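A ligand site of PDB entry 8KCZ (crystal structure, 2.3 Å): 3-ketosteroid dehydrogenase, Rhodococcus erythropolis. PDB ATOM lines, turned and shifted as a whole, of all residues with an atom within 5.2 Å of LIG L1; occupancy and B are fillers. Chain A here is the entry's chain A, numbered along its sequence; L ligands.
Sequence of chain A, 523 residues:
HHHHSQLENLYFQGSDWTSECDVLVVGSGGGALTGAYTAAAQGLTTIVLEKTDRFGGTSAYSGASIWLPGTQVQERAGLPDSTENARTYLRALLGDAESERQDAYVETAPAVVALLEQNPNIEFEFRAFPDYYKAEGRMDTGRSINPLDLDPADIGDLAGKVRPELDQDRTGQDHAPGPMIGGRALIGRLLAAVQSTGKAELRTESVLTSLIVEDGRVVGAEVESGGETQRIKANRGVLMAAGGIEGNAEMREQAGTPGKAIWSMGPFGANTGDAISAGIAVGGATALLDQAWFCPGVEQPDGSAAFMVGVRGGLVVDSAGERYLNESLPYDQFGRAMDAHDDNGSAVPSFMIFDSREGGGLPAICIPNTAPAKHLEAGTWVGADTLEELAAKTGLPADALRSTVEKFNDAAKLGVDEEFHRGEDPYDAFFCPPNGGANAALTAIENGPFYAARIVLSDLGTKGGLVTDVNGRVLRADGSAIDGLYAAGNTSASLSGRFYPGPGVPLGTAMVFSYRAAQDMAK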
ATOM      1  N   GLY A  63     -12.666  16.126  -8.592  1.00  0.00           N
ATOM      2  CA  GLY A  63     -11.779  16.884  -9.500  1.00  0.00           C
ATOM      3  C   GLY A  63     -10.324  16.555  -9.240  1.00  0.00           C
ATOM      4  O   GLY A  63      -9.440  17.143  -9.895  1.00  0.00           O
ATOM      5  N   SER A  65      -8.391  17.295  -6.985  1.00  0.00           N
ATOM      6  CA  SER A  65      -7.560  18.345  -6.368  1.00  0.00           C
ATOM      7  C   SER A  65      -7.081  17.751  -5.033  1.00  0.00           C
ATOM      8  O   SER A  65      -7.867  17.125  -4.317  1.00  0.00           O
ATOM      9  CB  SER A  65      -8.327  19.666  -6.299  1.00  0.00           C
ATOM     10  OG  SER A  65      -7.728  20.547  -5.382  1.00  0.00           O
ATOM     11  N   PHE A 129      -6.615  26.868  -7.208  1.00  0.00           N
ATOM     12  CA  PHE A 129      -7.968  26.793  -6.626  1.00  0.00           C
ATOM     13  C   PHE A 129      -7.803  27.350  -5.214  1.00  0.00           C
ATOM     14  O   PHE A 129      -6.974  26.842  -4.460  1.00  0.00           O
ATOM     15  CB  PHE A 129      -8.491  25.342  -6.707  1.00  0.00           C
ATOM     16  CG  PHE A 129      -9.992  25.269  -6.798  1.00  0.00           C
ATOM     17  CD1 PHE A 129     -10.788  25.389  -5.664  1.00  0.00           C
ATOM     18  CD2 PHE A 129     -10.629  25.097  -8.027  1.00  0.00           C
ATOM     19  CE1 PHE A 129     -12.177  25.344  -5.748  1.00  0.00           C
ATOM     20  CE2 PHE A 129     -12.017  25.075  -8.111  1.00  0.00           C
ATOM     21  CZ  PHE A 129     -12.784  25.184  -6.972  1.00  0.00           C
ATOM     22  N   TYR A 132      -9.883  28.178   1.509  1.00  0.00           N
ATOM     23  CA  TYR A 132     -11.317  28.509   1.745  1.00  0.00           C
ATOM     24  C   TYR A 132     -11.534  29.455   2.953  1.00  0.00           C
ATOM     25  O   TYR A 132     -12.671  29.942   3.078  1.00  0.00           O
ATOM     26  CB  TYR A 132     -12.120  27.222   1.947  1.00  0.00           C
ATOM     27  CG  TYR A 132     -12.154  26.257   0.790  1.00  0.00           C
ATOM     28  CD1 TYR A 132     -11.887  26.665  -0.506  1.00  0.00           C
ATOM     29  CD2 TYR A 132     -12.534  24.930   0.987  1.00  0.00           C
ATOM     30  CE1 TYR A 132     -11.955  25.786  -1.573  1.00  0.00           C
ATOM     31  CE2 TYR A 132     -12.600  24.028  -0.070  1.00  0.00           C
ATOM     32  CZ  TYR A 132     -12.319  24.454  -1.369  1.00  0.00           C
ATOM     33  OH  TYR A 132     -12.397  23.615  -2.444  1.00  0.00           O
ATOM     34  N   PHE A 307     -24.178  18.677  -6.758  1.00  0.00           N
ATOM     35  CA  PHE A 307     -23.171  19.573  -6.128  1.00  0.00           C
ATOM     36  C   PHE A 307     -23.211  20.928  -6.840  1.00  0.00           C
ATOM     37  O   PHE A 307     -23.011  20.913  -8.066  1.00  0.00           O
ATOM     38  CB  PHE A 307     -21.812  18.908  -6.239  1.00  0.00           C
ATOM     39  CG  PHE A 307     -20.652  19.670  -5.663  1.00  0.00           C
ATOM     40  CD1 PHE A 307     -20.853  20.635  -4.672  1.00  0.00           C
ATOM     41  CD2 PHE A 307     -19.363  19.389  -6.062  1.00  0.00           C
ATOM     42  CE1 PHE A 307     -19.775  21.269  -4.080  1.00  0.00           C
ATOM     43  CE2 PHE A 307     -18.291  20.055  -5.479  1.00  0.00           C
ATOM     44  CZ  PHE A 307     -18.497  21.007  -4.488  1.00  0.00           C
ATOM     45  N   VAL A 309     -21.387  24.362  -7.148  1.00  0.00           N
ATOM     46  CA  VAL A 309     -20.026  24.899  -6.829  1.00  0.00           C
ATOM     47  C   VAL A 309     -19.734  26.057  -7.806  1.00  0.00           C
ATOM     48  O   VAL A 309     -20.381  26.117  -8.877  1.00  0.00           O
ATOM     49  CB  VAL A 309     -18.965  23.774  -6.874  1.00  0.00           C
ATOM     50  CG1 VAL A 309     -18.777  23.209  -8.276  1.00  0.00           C
ATOM     51  CG2 VAL A 309     -17.615  24.239  -6.329  1.00  0.00           C
ATOM     52  N   TYR A 331     -18.332  25.975  -0.427  1.00  0.00           N
ATOM     53  CA  TYR A 331     -19.496  25.054  -0.331  1.00  0.00           C
ATOM     54  C   TYR A 331     -19.719  24.456   1.076  1.00  0.00           C
ATOM     55  O   TYR A 331     -20.889  24.294   1.478  1.00  0.00           O
ATOM     56  CB  TYR A 331     -19.368  23.953  -1.390  1.00  0.00           C
ATOM     57  CG  TYR A 331     -18.001  23.360  -1.513  1.00  0.00           C
ATOM     58  CD1 TYR A 331     -17.038  23.923  -2.337  1.00  0.00           C
ATOM     59  CD2 TYR A 331     -17.670  22.214  -0.817  1.00  0.00           C
ATOM     60  CE1 TYR A 331     -15.774  23.360  -2.459  1.00  0.00           C
ATOM     61  CE2 TYR A 331     -16.409  21.647  -0.907  1.00  0.00           C
ATOM     62  CZ  TYR A 331     -15.461  22.215  -1.739  1.00  0.00           C
ATOM     63  OH  TYR A 331     -14.225  21.652  -1.773  1.00  0.00           O
ATOM     64  N   ILE A 365     -21.683  25.972 -11.460  1.00  0.00           N
ATOM     65  CA  ILE A 365     -21.432  24.565 -11.893  1.00  0.00           C
ATOM     66  C   ILE A 365     -22.330  23.633 -11.056  1.00  0.00           C
ATOM     67  O   ILE A 365     -22.286  23.667  -9.798  1.00  0.00           O
ATOM     68  CB  ILE A 365     -19.932  24.217 -11.786  1.00  0.00           C
ATOM     69  CG1 ILE A 365     -19.097  25.277 -12.528  1.00  0.00           C
ATOM     70  CG2 ILE A 365     -19.644  22.823 -12.288  1.00  0.00           C
ATOM     71  CD1 ILE A 365     -17.671  25.395 -12.033  1.00  0.00           C
ATOM     72  N   ILE A 367     -23.171  19.533 -10.661  1.00  0.00           N
ATOM     73  CA  ILE A 367     -22.621  18.183 -10.981  1.00  0.00           C
ATOM     74  C   ILE A 367     -23.511  17.139 -10.310  1.00  0.00           C
ATOM     75  O   ILE A 367     -23.493  17.000  -9.090  1.00  0.00           O
ATOM     76  CB  ILE A 367     -21.152  18.108 -10.558  1.00  0.00           C
ATOM     77  CG1 ILE A 367     -20.371  19.338 -11.053  1.00  0.00           C
ATOM     78  CG2 ILE A 367     -20.481  16.804 -11.005  1.00  0.00           C
ATOM     79  CD1 ILE A 367     -18.926  19.397 -10.542  1.00  0.00           C
ATOM     80  N   LEU A 460     -20.440  15.641   0.162  1.00  0.00           N
ATOM     81  CA  LEU A 460     -19.427  14.958  -0.654  1.00  0.00           C
ATOM     82  C   LEU A 460     -18.861  13.787   0.146  1.00  0.00           C
ATOM     83  O   LEU A 460     -17.631  13.538   0.035  1.00  0.00           O
ATOM     84  CB  LEU A 460     -18.311  15.958  -0.975  1.00  0.00           C
ATOM     85  CG  LEU A 460     -18.735  17.245  -1.630  1.00  0.00           C
ATOM     86  CD1 LEU A 460     -17.511  18.070  -1.933  1.00  0.00           C
ATOM     87  CD2 LEU A 460     -19.520  16.988  -2.901  1.00  0.00           C
ATOM     88  N   TYR A 500     -13.481  22.540   6.567  1.00  0.00           N
ATOM     89  CA  TYR A 500     -13.011  22.164   5.221  1.00  0.00           C
ATOM     90  C   TYR A 500     -11.979  23.211   4.816  1.00  0.00           C
ATOM     91  O   TYR A 500     -12.306  24.226   4.230  1.00  0.00           O
ATOM     92  CB  TYR A 500     -14.229  22.018   4.295  1.00  0.00           C
ATOM     93  CG  TYR A 500     -14.047  21.158   3.065  1.00  0.00           C
ATOM     94  CD1 TYR A 500     -12.856  21.119   2.351  1.00  0.00           C
ATOM     95  CD2 TYR A 500     -15.109  20.433   2.560  1.00  0.00           C
ATOM     96  CE1 TYR A 500     -12.728  20.372   1.173  1.00  0.00           C
ATOM     97  CE2 TYR A 500     -14.995  19.655   1.406  1.00  0.00           C
ATOM     98  CZ  TYR A 500     -13.808  19.647   0.693  1.00  0.00           C
ATOM     99  OH  TYR A 500     -13.733  18.907  -0.453  1.00  0.00           O
ATOM    100  N   GLY A 502      -9.406  23.697   2.702  1.00  0.00           N
ATOM    101  CA  GLY A 502      -9.102  24.055   1.306  1.00  0.00           C
ATOM    102  C   GLY A 502      -9.348  22.908   0.344  1.00  0.00           C
ATOM    103  O   GLY A 502      -9.647  21.792   0.771  1.00  0.00           O
ATOM    104  N   PRO A 503      -9.180  23.131  -0.985  1.00  0.00           N
ATOM    105  CA  PRO A 503      -9.495  22.098  -1.962  1.00  0.00           C
ATOM    106  C   PRO A 503      -8.534  20.921  -1.732  1.00  0.00           C
ATOM    107  O   PRO A 503      -7.351  21.151  -1.564  1.00  0.00           O
ATOM    108  CB  PRO A 503      -9.252  22.798  -3.311  1.00  0.00           C
ATOM    109  CG  PRO A 503      -8.143  23.804  -2.976  1.00  0.00           C
ATOM    110  CD  PRO A 503      -8.546  24.308  -1.613  1.00  0.00           C
ATOM    111  N   GLY A 504      -9.052  19.703  -1.690  1.00  0.00           N
ATOM    112  CA  GLY A 504      -8.201  18.503  -1.723  1.00  0.00           C
ATOM    113  C   GLY A 504      -7.877  17.978  -0.335  1.00  0.00           C
ATOM    114  O   GLY A 504      -7.054  17.074  -0.258  1.00  0.00           O
ATOM    115  N   VAL A 505      -8.493  18.494   0.725  1.00  0.00           N
ATOM    116  CA  VAL A 505      -8.214  18.006   2.092  1.00  0.00           C
ATOM    117  C   VAL A 505      -8.767  16.591   2.282  1.00  0.00           C
ATOM    118  O   VAL A 505      -8.132  15.776   2.920  1.00  0.00           O
ATOM    119  CB  VAL A 505      -8.729  18.962   3.177  1.00  0.00           C
ATOM    120  CG1 VAL A 505      -8.711  18.312   4.545  1.00  0.00           C
ATOM    121  CG2 VAL A 505      -7.899  20.237   3.204  1.00  0.00           C
ATOM    122  N   PRO A 506      -9.986  16.242   1.824  1.00  0.00           N
ATOM    123  CA  PRO A 506     -10.473  14.865   1.930  1.00  0.00           C
ATOM    124  C   PRO A 506      -9.488  13.879   1.269  1.00  0.00           C
ATOM    125  O   PRO A 506      -9.046  12.986   1.935  1.00  0.00           O
ATOM    126  CB  PRO A 506     -11.860  14.903   1.265  1.00  0.00           C
ATOM    127  CG  PRO A 506     -12.292  16.330   1.460  1.00  0.00           C
ATOM    128  CD  PRO A 506     -11.012  17.127   1.258  1.00  0.00           C
HETATM  129  C1  LIG L   1     -14.289  19.913  -4.963  1.00  0.00           C
HETATM  130  C2  LIG L   1     -13.581  20.896  -5.843  1.00  0.00           C
HETATM  131  C3  LIG L   1     -15.122  20.228  -7.821  1.00  0.00           C
HETATM  132  C4  LIG L   1     -15.245  19.862  -9.300  1.00  0.00           C
HETATM  133  C5  LIG L   1     -14.478  20.848 -10.162  1.00  0.00           C
HETATM  134  C6  LIG L   1     -13.007  20.839  -9.738  1.00  0.00           C
HETATM  135  C7  LIG L   1     -12.257  21.527 -10.885  1.00  0.00           C
HETATM  136  C8  LIG L   1     -13.044  21.092 -12.137  1.00  0.00           C
HETATM  137  C9  LIG L   1     -14.339  20.478 -11.633  1.00  0.00           C
HETATM  138  C10 LIG L   1     -15.095  22.254 -10.153  1.00  0.00           C
HETATM  139  C11 LIG L   1     -14.239  22.267  -5.561  1.00  0.00           C
HETATM  140  C12 LIG L   1     -13.798  19.454  -3.813  1.00  0.00           C
HETATM  141  C13 LIG L   1     -12.424  19.682  -3.429  1.00  0.00           C
HETATM  142  C14 LIG L   1     -11.605  20.394  -4.395  1.00  0.00           C
HETATM  143  C15 LIG L   1     -12.108  20.973  -5.491  1.00  0.00           C
HETATM  144  C16 LIG L   1     -11.220  21.736  -6.441  1.00  0.00           C
HETATM  145  C17 LIG L   1     -11.373  21.264  -7.874  1.00  0.00           C
HETATM  146  C18 LIG L   1     -12.838  21.307  -8.298  1.00  0.00           C
HETATM  147  C19 LIG L   1     -13.683  20.431  -7.338  1.00  0.00           C
HETATM  148  O1  LIG L   1     -11.977  19.297  -2.330  1.00  0.00           O
HETATM  149  O2  LIG L   1     -15.116  19.784 -12.267  1.00  0.00           O
HETATM  150  P1  LG2 L   2     -14.521   6.641  -1.756  1.00  0.00           P
HETATM  151  O1  LG2 L   2     -13.597   7.403  -2.642  1.00  0.00           O
HETATM  152  O2  LG2 L   2     -16.005   6.739  -2.033  1.00  0.00           O
HETATM  153  O3  LG2 L   2     -14.055   5.118  -1.725  1.00  0.00           O
HETATM  154  C1  LG2 L   2     -14.848   4.125  -1.011  1.00  0.00           C
HETATM  155  C2  LG2 L   2     -14.919   2.842  -1.806  1.00  0.00           C
HETATM  156  O4  LG2 L   2     -15.128   1.726  -0.877  1.00  0.00           O
HETATM  157  C3  LG2 L   2     -16.071   2.788  -2.806  1.00  0.00           C
HETATM  158  O5  LG2 L   2     -15.693   2.343  -4.103  1.00  0.00           O
HETATM  159  C4  LG2 L   2     -17.053   1.806  -2.166  1.00  0.00           C
HETATM  160  O6  LG2 L   2     -17.837   1.132  -3.125  1.00  0.00           O
HETATM  161  C5  LG2 L   2     -16.095   0.873  -1.433  1.00  0.00           C
HETATM  162  N1  LG2 L   2     -16.732   0.093  -0.392  1.00  0.00           N
HETATM  163  C6  LG2 L   2     -17.734   0.511   0.471  1.00  0.00           C
HETATM  164  N2  LG2 L   2     -18.104  -0.425   1.303  1.00  0.00           N
HETATM  165  C7  LG2 L   2     -17.284  -1.510   0.991  1.00  0.00           C
HETATM  166  C8  LG2 L   2     -17.219  -2.803   1.526  1.00  0.00           C
HETATM  167  N3  LG2 L   2     -18.029  -3.224   2.494  1.00  0.00           N
HETATM  168  N4  LG2 L   2     -16.294  -3.631   0.991  1.00  0.00           N
HETATM  169  C9  LG2 L   2     -15.514  -3.187  -0.012  1.00  0.00           C
HETATM  170  N5  LG2 L   2     -15.514  -2.012  -0.612  1.00  0.00           N
HETATM  171  C10 LG2 L   2     -16.433  -1.207  -0.048  1.00  0.00           C
HETATM  172  N6  LG2 L   2     -12.187  15.868  -2.476  1.00  0.00           N
HETATM  173  C11 LG2 L   2     -10.921  16.262  -2.690  1.00  0.00           C
HETATM  174  O7  LG2 L   2     -10.052  16.124  -1.818  1.00  0.00           O
HETATM  175  N7  LG2 L   2     -10.537  16.863  -3.845  1.00  0.00           N
HETATM  176  C12 LG2 L   2     -11.421  17.204  -4.824  1.00  0.00           C
HETATM  177  O8  LG2 L   2     -10.983  17.717  -5.857  1.00  0.00           O
HETATM  178  C13 LG2 L   2     -12.768  16.745  -4.665  1.00  0.00           C
HETATM  179  N8  LG2 L   2     -13.655  16.991  -5.593  1.00  0.00           N
HETATM  180  C14 LG2 L   2     -14.904  16.435  -5.455  1.00  0.00           C
HETATM  181  C15 LG2 L   2     -15.817  16.594  -6.502  1.00  0.00           C
HETATM  182  C16 LG2 L   2     -17.034  15.957  -6.504  1.00  0.00           C
HETATM  183  C17 LG2 L   2     -17.972  16.161  -7.678  1.00  0.00           C
HETATM  184  C18 LG2 L   2     -17.390  15.154  -5.398  1.00  0.00           C
HETATM  185  C19 LG2 L   2     -18.741  14.503  -5.322  1.00  0.00           C
HETATM  186  C20 LG2 L   2     -16.548  15.100  -4.295  1.00  0.00           C
HETATM  187  C21 LG2 L   2     -15.276  15.678  -4.325  1.00  0.00           C
HETATM  188  N9  LG2 L   2     -14.361  15.564  -3.279  1.00  0.00           N
HETATM  189  C22 LG2 L   2     -13.074  16.061  -3.425  1.00  0.00           C
HETATM  190  C23 LG2 L   2     -14.687  14.764  -2.077  1.00  0.00           C
HETATM  191  C24 LG2 L   2     -14.077  13.403  -2.124  1.00  0.00           C
HETATM  192  O9  LG2 L   2     -14.388  12.800  -3.414  1.00  0.00           O
HETATM  193  C25 LG2 L   2     -14.538  12.411  -1.040  1.00  0.00           C
HETATM  194  O10 LG2 L   2     -14.882  12.954   0.210  1.00  0.00           O
HETATM  195  C26 LG2 L   2     -13.407  11.435  -0.832  1.00  0.00           C
HETATM  196  O11 LG2 L   2     -12.968  10.983  -2.121  1.00  0.00           O
HETATM  197  C27 LG2 L   2     -13.832  10.255  -0.012  1.00  0.00           C
HETATM  198  O12 LG2 L   2     -12.936   9.167  -0.289  1.00  0.00           O
HETATM  199  P2  LG2 L   2     -13.104   7.804   0.548  1.00  0.00           P
HETATM  200  O13 LG2 L   2     -11.864   7.063   0.337  1.00  0.00           O
HETATM  201  O14 LG2 L   2     -13.552   8.153   1.940  1.00  0.00           O
HETATM  202  O15 LG2 L   2     -14.302   7.103  -0.245  1.00  0.00           O
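An oxygen (O1) of LIG L1 sits at hydrogen-bond distance from the side-chain hydroxyl (OH) of Tyr 500, 2.6 Å away. An oxygen (O1) of LIG L1 sits at hydrogen-bond distance from the backbone NH (N) of Gly 504 (3.0 Å). The side-chain hydroxyl (OH) of Tyr 331 lies close to an oxygen (O1) of LIG L1 (3.3 Å). The backbone NH of Ser 65 lies within hydrogen-bond range of an oxygen (O8) of LG2 L2 (2.9 Å). A nitrogen (N7) of LG2 L2 lies within hydrogen-bond range of the backbone carbonyl oxygen (O) of Ser 65 (2.7 Å). The backbone NH of Gly 63 is in hydrogen-bond range of a nitrogen (N8) of LG2 L2, 3.3 Å away. An oxygen (O10) of LG2 L2 lies within hydrogen-bond range of the backbone carbonyl oxygen of Leu 460, at 2.8 Å.
O1 of LIG L1 sits at hydrogen-bond distance from N7 of LG2 L2 (3.2 Å).
The side-chain hydroxyl (OH) of Tyr 500 is in hydrogen-bond range of the side-chain hydroxyl (OH) of Tyr 331 (3.1 Å). The side-chain hydroxyl (OH) of Tyr 331 sits at hydrogen-bond distance from the side-chain hydroxyl (OH) of Tyr 132 (2.8 Å). The backbone carbonyl oxygen (O) of Phe 307 lies within hydrogen-bond range of the backbone NH (N) of Ile 367 (2.9 Å). N of Val 309 is in hydrogen-bond range of O of Ile 365, 2.9 Å away.
Ser 65 touches LIG L1 (CB to C16, 3.6 Å). Phe 129 touches LIG L1 (CZ to C11, 3.6 Å). OH of Tyr 132 touches C14 of LIG L1 (3.8 Å). Phe 307 touches LIG L1. CG2 of Val 309 touches C11 of LIG L1, 3.98 Å away. Ile 367 touches LIG L1. Pro 503 touches LIG L1. Ten residues have an atom within 4 Å of LIG L1: Ser 65, Phe 129, Tyr 132, Phe 307, Val 309, Tyr 331, Ile 367, Tyr 500, Pro 503 and Gly 504.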
